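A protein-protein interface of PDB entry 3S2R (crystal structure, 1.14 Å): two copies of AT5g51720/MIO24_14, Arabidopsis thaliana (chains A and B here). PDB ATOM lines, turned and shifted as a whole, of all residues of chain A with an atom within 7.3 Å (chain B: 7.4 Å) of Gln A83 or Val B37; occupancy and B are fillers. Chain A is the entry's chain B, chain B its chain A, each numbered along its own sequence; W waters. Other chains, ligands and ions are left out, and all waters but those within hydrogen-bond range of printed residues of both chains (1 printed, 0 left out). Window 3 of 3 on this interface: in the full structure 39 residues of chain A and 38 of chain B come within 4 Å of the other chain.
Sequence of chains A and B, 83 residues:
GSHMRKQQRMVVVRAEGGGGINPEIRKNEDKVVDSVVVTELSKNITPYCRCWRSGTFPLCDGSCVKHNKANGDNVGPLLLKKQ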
ATOM      1  N   LYS A  43     -27.151  -2.346 -14.172  1.00  0.00           N
ATOM      2  CA  LYS A  43     -27.502  -3.208 -13.043  1.00  0.00           C
ATOM      3  C   LYS A  43     -26.660  -2.760 -11.820  1.00  0.00           C
ATOM      4  O   LYS A  43     -25.575  -2.161 -11.948  1.00  0.00           O
ATOM      5  CB  LYS A  43     -27.168  -4.681 -13.369  1.00  0.00           C
ATOM      6  CG  LYS A  43     -28.030  -5.279 -14.481  1.00  0.00           C
ATOM      7  CD  LYS A  43     -27.727  -6.777 -14.663  1.00  0.00           C
ATOM      8  CE  LYS A  43     -26.409  -6.976 -15.362  1.00  0.00           C
ATOM      9  NZ  LYS A  43     -26.274  -8.421 -15.628  1.00  0.00           N
ATOM     10  N   ASN A  44     -27.113  -3.130 -10.629  1.00  0.00           N
ATOM     11  CA  ASN A  44     -26.301  -2.851  -9.468  1.00  0.00           C
ATOM     12  C   ASN A  44     -24.994  -3.632  -9.463  1.00  0.00           C
ATOM     13  O   ASN A  44     -23.958  -3.108  -9.043  1.00  0.00           O
ATOM     14  CB  ASN A  44     -27.071  -3.105  -8.164  1.00  0.00           C
ATOM     15  CG  ASN A  44     -26.283  -2.747  -6.972  1.00  0.00           C
ATOM     16  OD1 ASN A  44     -25.817  -1.597  -6.858  1.00  0.00           O
ATOM     17  ND2 ASN A  44     -26.035  -3.722  -6.116  1.00  0.00           N
ATOM     18  N   ILE A  45     -25.018  -4.896  -9.937  1.00  0.00           N
ATOM     19  CA  ILE A  45     -23.846  -5.750 -10.002  1.00  0.00           C
ATOM     20  C   ILE A  45     -23.695  -6.274 -11.426  1.00  0.00           C
ATOM     21  O   ILE A  45     -24.634  -6.823 -11.992  1.00  0.00           O
ATOM     22  CB  ILE A  45     -23.918  -6.923  -9.000  1.00  0.00           C
ATOM     23  CG1 ILE A  45     -24.168  -6.395  -7.581  1.00  0.00           C
ATOM     24  CG2 ILE A  45     -22.610  -7.708  -9.096  1.00  0.00           C
ATOM     25  CD1 ILE A  45     -24.271  -7.514  -6.534  1.00  0.00           C
ATOM     26  N   LEU A  79     -16.635  -8.235  -9.956  1.00  0.00           N
ATOM     27  CA  LEU A  79     -17.990  -7.740  -9.812  1.00  0.00           C
ATOM     28  C   LEU A  79     -17.959  -6.237  -9.707  1.00  0.00           C
ATOM     29  O   LEU A  79     -17.421  -5.708  -8.734  1.00  0.00           O
ATOM     30  CB  LEU A  79     -18.682  -8.308  -8.542  1.00  0.00           C
ATOM     31  CG  LEU A  79     -18.653  -9.834  -8.440  1.00  0.00           C
ATOM     32  CD1 LEU A  79     -19.440 -10.286  -7.212  1.00  0.00           C
ATOM     33  CD2 LEU A  79     -19.235 -10.521  -9.691  1.00  0.00           C
ATOM     34  N   LEU A  80     -18.496  -5.538 -10.694  1.00  0.00           N
ATOM     35  CA  LEU A  80     -18.589  -4.092 -10.638  1.00  0.00           C
ATOM     36  C   LEU A  80     -19.909  -3.701 -10.019  1.00  0.00           C
ATOM     37  O   LEU A  80     -20.971  -4.119 -10.530  1.00  0.00           O
ATOM     38  CB  LEU A  80     -18.423  -3.442 -12.028  1.00  0.00           C
ATOM     39  CG  LEU A  80     -17.150  -3.823 -12.805  1.00  0.00           C
ATOM     40  CD1 LEU A  80     -17.089  -3.018 -14.070  1.00  0.00           C
ATOM     41  CD2 LEU A  80     -15.882  -3.622 -11.942  1.00  0.00           C
ATOM     42  N   LYS A  81     -19.854  -2.921  -8.937  1.00  0.00           N
ATOM     43  CA  LYS A  81     -21.024  -2.616  -8.155  1.00  0.00           C
ATOM     44  C   LYS A  81     -21.273  -1.128  -8.108  1.00  0.00           C
ATOM     45  O   LYS A  81     -20.360  -0.332  -7.920  1.00  0.00           O
ATOM     46  CB  LYS A  81     -20.851  -3.142  -6.727  1.00  0.00           C
ATOM     47  CG  LYS A  81     -20.594  -4.597  -6.620  1.00  0.00           C
ATOM     48  CD  LYS A  81     -20.625  -5.091  -5.197  1.00  0.00           C
ATOM     49  CE  LYS A  81     -20.481  -6.622  -5.135  1.00  0.00           C
ATOM     50  NZ  LYS A  81     -20.493  -7.055  -3.731  1.00  0.00           N
ATOM     51  N   LYS A  82     -22.535  -0.768  -8.266  1.00  0.00           N
ATOM     52  CA  LYS A  82     -22.925   0.648  -8.176  1.00  0.00           C
ATOM     53  C   LYS A  82     -23.007   1.126  -6.726  1.00  0.00           C
ATOM     54  O   LYS A  82     -22.898   2.328  -6.491  1.00  0.00           O
ATOM     55  CB  LYS A  82     -24.259   0.906  -8.890  1.00  0.00           C
ATOM     56  CG  LYS A  82     -24.236   0.704 -10.397  1.00  0.00           C
ATOM     57  CD  LYS A  82     -25.639   1.078 -10.945  1.00  0.00           C
ATOM     58  CE  LYS A  82     -25.835   1.058 -12.366  1.00  0.00           C
ATOM     59  NZ  LYS A  82     -27.097   1.826 -12.564  1.00  0.00           N
ATOM     60  N   GLN A  83     -23.287   0.208  -5.801  1.00  0.00           N
ATOM     61  CA  GLN A  83     -23.494   0.482  -4.399  1.00  0.00           C
ATOM     62  C   GLN A  83     -22.807  -0.605  -3.620  1.00  0.00           C
ATOM     63  O   GLN A  83     -22.634  -1.725  -4.064  1.00  0.00           O
ATOM     64  CB  GLN A  83     -25.003   0.458  -4.075  1.00  0.00           C
ATOM     65  CG  GLN A  83     -25.865   1.514  -4.799  1.00  0.00           C
ATOM     66  CD  GLN A  83     -25.591   2.956  -4.338  1.00  0.00           C
ATOM     67  OE1 GLN A  83     -25.064   3.193  -3.227  1.00  0.00           O
ATOM     68  NE2 GLN A  83     -25.958   3.924  -5.189  1.00  0.00           N
ATOM     69  N   SER B  35     -14.678  -7.682  -5.797  1.00  0.00           N
ATOM     70  CA  SER B  35     -15.722  -6.667  -6.016  1.00  0.00           C
ATOM     71  C   SER B  35     -15.139  -5.275  -6.013  1.00  0.00           C
ATOM     72  O   SER B  35     -14.204  -5.000  -5.225  1.00  0.00           O
ATOM     73  CB  SER B  35     -16.781  -6.712  -4.906  1.00  0.00           C
ATOM     74  OG  SER B  35     -17.532  -7.918  -5.022  1.00  0.00           O
ATOM     75  N   VAL B  36     -15.738  -4.385  -6.811  1.00  0.00           N
ATOM     76  CA  VAL B  36     -15.360  -2.985  -6.844  1.00  0.00           C
ATOM     77  C   VAL B  36     -16.629  -2.175  -6.720  1.00  0.00           C
ATOM     78  O   VAL B  36     -17.492  -2.305  -7.565  1.00  0.00           O
ATOM     79  CB  VAL B  36     -14.628  -2.641  -8.184  1.00  0.00           C
ATOM     80  CG1 VAL B  36     -14.298  -1.136  -8.221  1.00  0.00           C
ATOM     81  CG2 VAL B  36     -13.398  -3.544  -8.390  1.00  0.00           C
ATOM     82  N   VAL B  37     -16.711  -1.321  -5.712  1.00  0.00           N
ATOM     83  CA  VAL B  37     -17.807  -0.350  -5.647  1.00  0.00           C
ATOM     84  C   VAL B  37     -17.288   0.867  -6.397  1.00  0.00           C
ATOM     85  O   VAL B  37     -16.334   1.527  -5.950  1.00  0.00           O
ATOM     86  CB  VAL B  37     -18.215  -0.042  -4.197  1.00  0.00           C
ATOM     87  CG1 VAL B  37     -19.217   1.103  -4.189  1.00  0.00           C
ATOM     88  CG2 VAL B  37     -18.759  -1.290  -3.559  1.00  0.00           C
ATOM     89  N   VAL B  38     -17.873   1.134  -7.560  1.00  0.00           N
ATOM     90  CA  VAL B  38     -17.212   2.043  -8.499  1.00  0.00           C
ATOM     91  C   VAL B  38     -17.109   3.487  -8.013  1.00  0.00           C
ATOM     92  O   VAL B  38     -16.204   4.217  -8.437  1.00  0.00           O
ATOM     93  CB  VAL B  38     -17.830   1.978  -9.881  1.00  0.00           C
ATOM     94  CG1 VAL B  38     -17.771   0.568 -10.436  1.00  0.00           C
ATOM     95  CG2 VAL B  38     -19.293   2.455  -9.865  1.00  0.00           C
ATOM     96  N   THR B  39     -17.967   3.893  -7.081  1.00  0.00           N
ATOM     97  CA  THR B  39     -17.891   5.236  -6.478  1.00  0.00           C
ATOM     98  C   THR B  39     -16.674   5.403  -5.563  1.00  0.00           C
ATOM     99  O   THR B  39     -16.319   6.522  -5.224  1.00  0.00           O
ATOM    100  CB  THR B  39     -19.150   5.529  -5.681  1.00  0.00           C
ATOM    101  OG1 THR B  39     -19.307   4.515  -4.693  1.00  0.00           O
ATOM    102  CG2 THR B  39     -20.377   5.579  -6.591  1.00  0.00           C
ATOM    103  N   GLU B  40     -16.005   4.306  -5.226  1.00  0.00           N
ATOM    104  CA  GLU B  40     -14.820   4.341  -4.368  1.00  0.00           C
ATOM    105  C   GLU B  40     -13.532   4.512  -5.155  1.00  0.00           C
ATOM    106  O   GLU B  40     -12.478   4.701  -4.560  1.00  0.00           O
ATOM    107  CB  GLU B  40     -14.748   3.095  -3.483  1.00  0.00           C
ATOM    108  CG  GLU B  40     -15.897   3.028  -2.557  1.00  0.00           C
ATOM    109  CD  GLU B  40     -15.924   1.807  -1.664  1.00  0.00           C
ATOM    110  OE1 GLU B  40     -15.152   0.863  -1.861  1.00  0.00           O
ATOM    111  OE2 GLU B  40     -16.780   1.794  -0.781  1.00  0.00           O
ATOM    112  N   LEU B  41     -13.567   4.373  -6.468  1.00  0.00           N
ATOM    113  CA  LEU B  41     -12.348   4.512  -7.263  1.00  0.00           C
ATOM    114  C   LEU B  41     -11.730   5.872  -7.125  1.00  0.00           C
ATOM    115  O   LEU B  41     -12.482   6.847  -6.957  1.00  0.00           O
ATOM    116  CB  LEU B  41     -12.688   4.279  -8.714  1.00  0.00           C
ATOM    117  CG  LEU B  41     -13.104   2.825  -9.066  1.00  0.00           C
ATOM    118  CD1 LEU B  41     -13.796   2.787 -10.386  1.00  0.00           C
ATOM    119  CD2 LEU B  41     -11.911   1.822  -8.998  1.00  0.00           C
ATOM    120  N   TYR B  48      -7.688  -3.210 -13.835  1.00  0.00           N
ATOM    121  CA  TYR B  48      -7.907  -4.430 -13.111  1.00  0.00           C
ATOM    122  C   TYR B  48      -7.348  -5.646 -13.895  1.00  0.00           C
ATOM    123  O   TYR B  48      -7.574  -5.746 -15.098  1.00  0.00           O
ATOM    124  CB  TYR B  48      -9.392  -4.615 -12.778  1.00  0.00           C
ATOM    125  CG  TYR B  48      -9.725  -3.884 -11.503  1.00  0.00           C
ATOM    126  CD1 TYR B  48      -9.788  -4.567 -10.285  1.00  0.00           C
ATOM    127  CD2 TYR B  48      -9.880  -2.496 -11.475  1.00  0.00           C
ATOM    128  CE1 TYR B  48     -10.017  -3.873  -9.074  1.00  0.00           C
ATOM    129  CE2 TYR B  48     -10.118  -1.812 -10.284  1.00  0.00           C
ATOM    130  CZ  TYR B  48     -10.171  -2.505  -9.095  1.00  0.00           C
ATOM    131  OH  TYR B  48     -10.385  -1.829  -7.918  1.00  0.00           O
ATOM    132  N   LEU B  80     -11.221   0.714 -15.647  1.00  0.00           N
ATOM    133  CA  LEU B  80     -12.406   1.346 -15.072  1.00  0.00           C
ATOM    134  C   LEU B  80     -12.186   2.864 -15.099  1.00  0.00           C
ATOM    135  O   LEU B  80     -11.267   3.372 -14.446  1.00  0.00           O
ATOM    136  CB  LEU B  80     -12.661   0.823 -13.652  1.00  0.00           C
ATOM    137  CG  LEU B  80     -12.790  -0.687 -13.481  1.00  0.00           C
ATOM    138  CD1 LEU B  80     -13.259  -0.971 -12.067  1.00  0.00           C
ATOM    139  CD2 LEU B  80     -13.800  -1.227 -14.491  1.00  0.00           C
HETATM  140  O   HOH W   1     -21.945   3.704  -4.262  1.00  0.00           O
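Among the printed residues, merely in contact across the chains: Leu A79 with Ser B35 (3.3 Å), Leu A80 with Val B36 (3.7 Å), Leu A80 with Leu B80 (3.7 Å), Lys A81 with Val B37 (3.4 Å) and Gln A83 with Val B37 (3.9 Å).
Ile A45 touches none of the printed residues of chain B.
Of the printed residues of chain B, Leu A79 touches Ser B35 (3.3 Å) and Val B36 (2.9 Å).
Of the printed residues of chain B, Leu A80 touches Val B36 and Leu B80.
Of the printed residues of chain B, Lys A81 touches Ser B35, Val B36, Val B37 and Val B38.
Gln A83 touches just one residue of chain B: Val B37.
Printed residues of chain A within 4 Å of Ser B35: Leu A79 (3.3 Å) and Lys A81 (3.2 Å).
Printed residues of chain A within 4 Å of Val B36: Leu A79 (2.9 Å), Leu A80 (3.7 Å) and Lys A81 (2.8 Å).
Of chain A, only Lys A81 and Gln A83 come within 4 Å of Val B37.
The nearest residue of chain B that does not touch Gln A83 is Val B38 (5.8 Å).
The nearest printed residue of chain B that does not touch Leu A80 is Val B38 (4.4 Å).
The side-chain amide oxygen (OD1) of Asn A44 lies within hydrogen-bond range of the backbone NH (N) of Gln A83, 3.3 Å away.
Water W1 lies within hydrogen-bond range of the backbone carbonyl oxygen of Lys A82 (2.8 Å), the side-chain hydroxyl of Thr B39 (2.8 Å) and the side-chain amide oxygen of Gln A83 (3.3 Å).
Of the 8 printed residues of chain A, 4 touch a printed residue of chain B.
Printed residues of chain B that touch a printed residue of chain A: Ser B35, Val B36, Val B37, Val B38 and Leu B80.
Among the printed residues, no Asp or Glu carboxylate lies within 4 Å of a Lys or Arg side-chain nitrogen of the other chain.
NZ of Lys A81 lies close to OG of Ser B35 (3.3 Å).
The backbone carbonyl oxygen (O) of Leu A79 is in hydrogen-bond range of the backbone NH (N) of Val B36 (2.9 Å).
O of Val B36 is in hydrogen-bond range of N of Lys A81, at 2.8 Å.
The backbone carbonyl oxygen of Lys A81 sits at hydrogen-bond distance from the backbone NH of Val B38 (2.9 Å).
Leu A80 touches its own counterpart, Leu B80.
Position printed for both chains: 80.
Of the 9 pairs that touch across the chains among the printed residues, 1 has its exchanged pair printed and touching as well.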
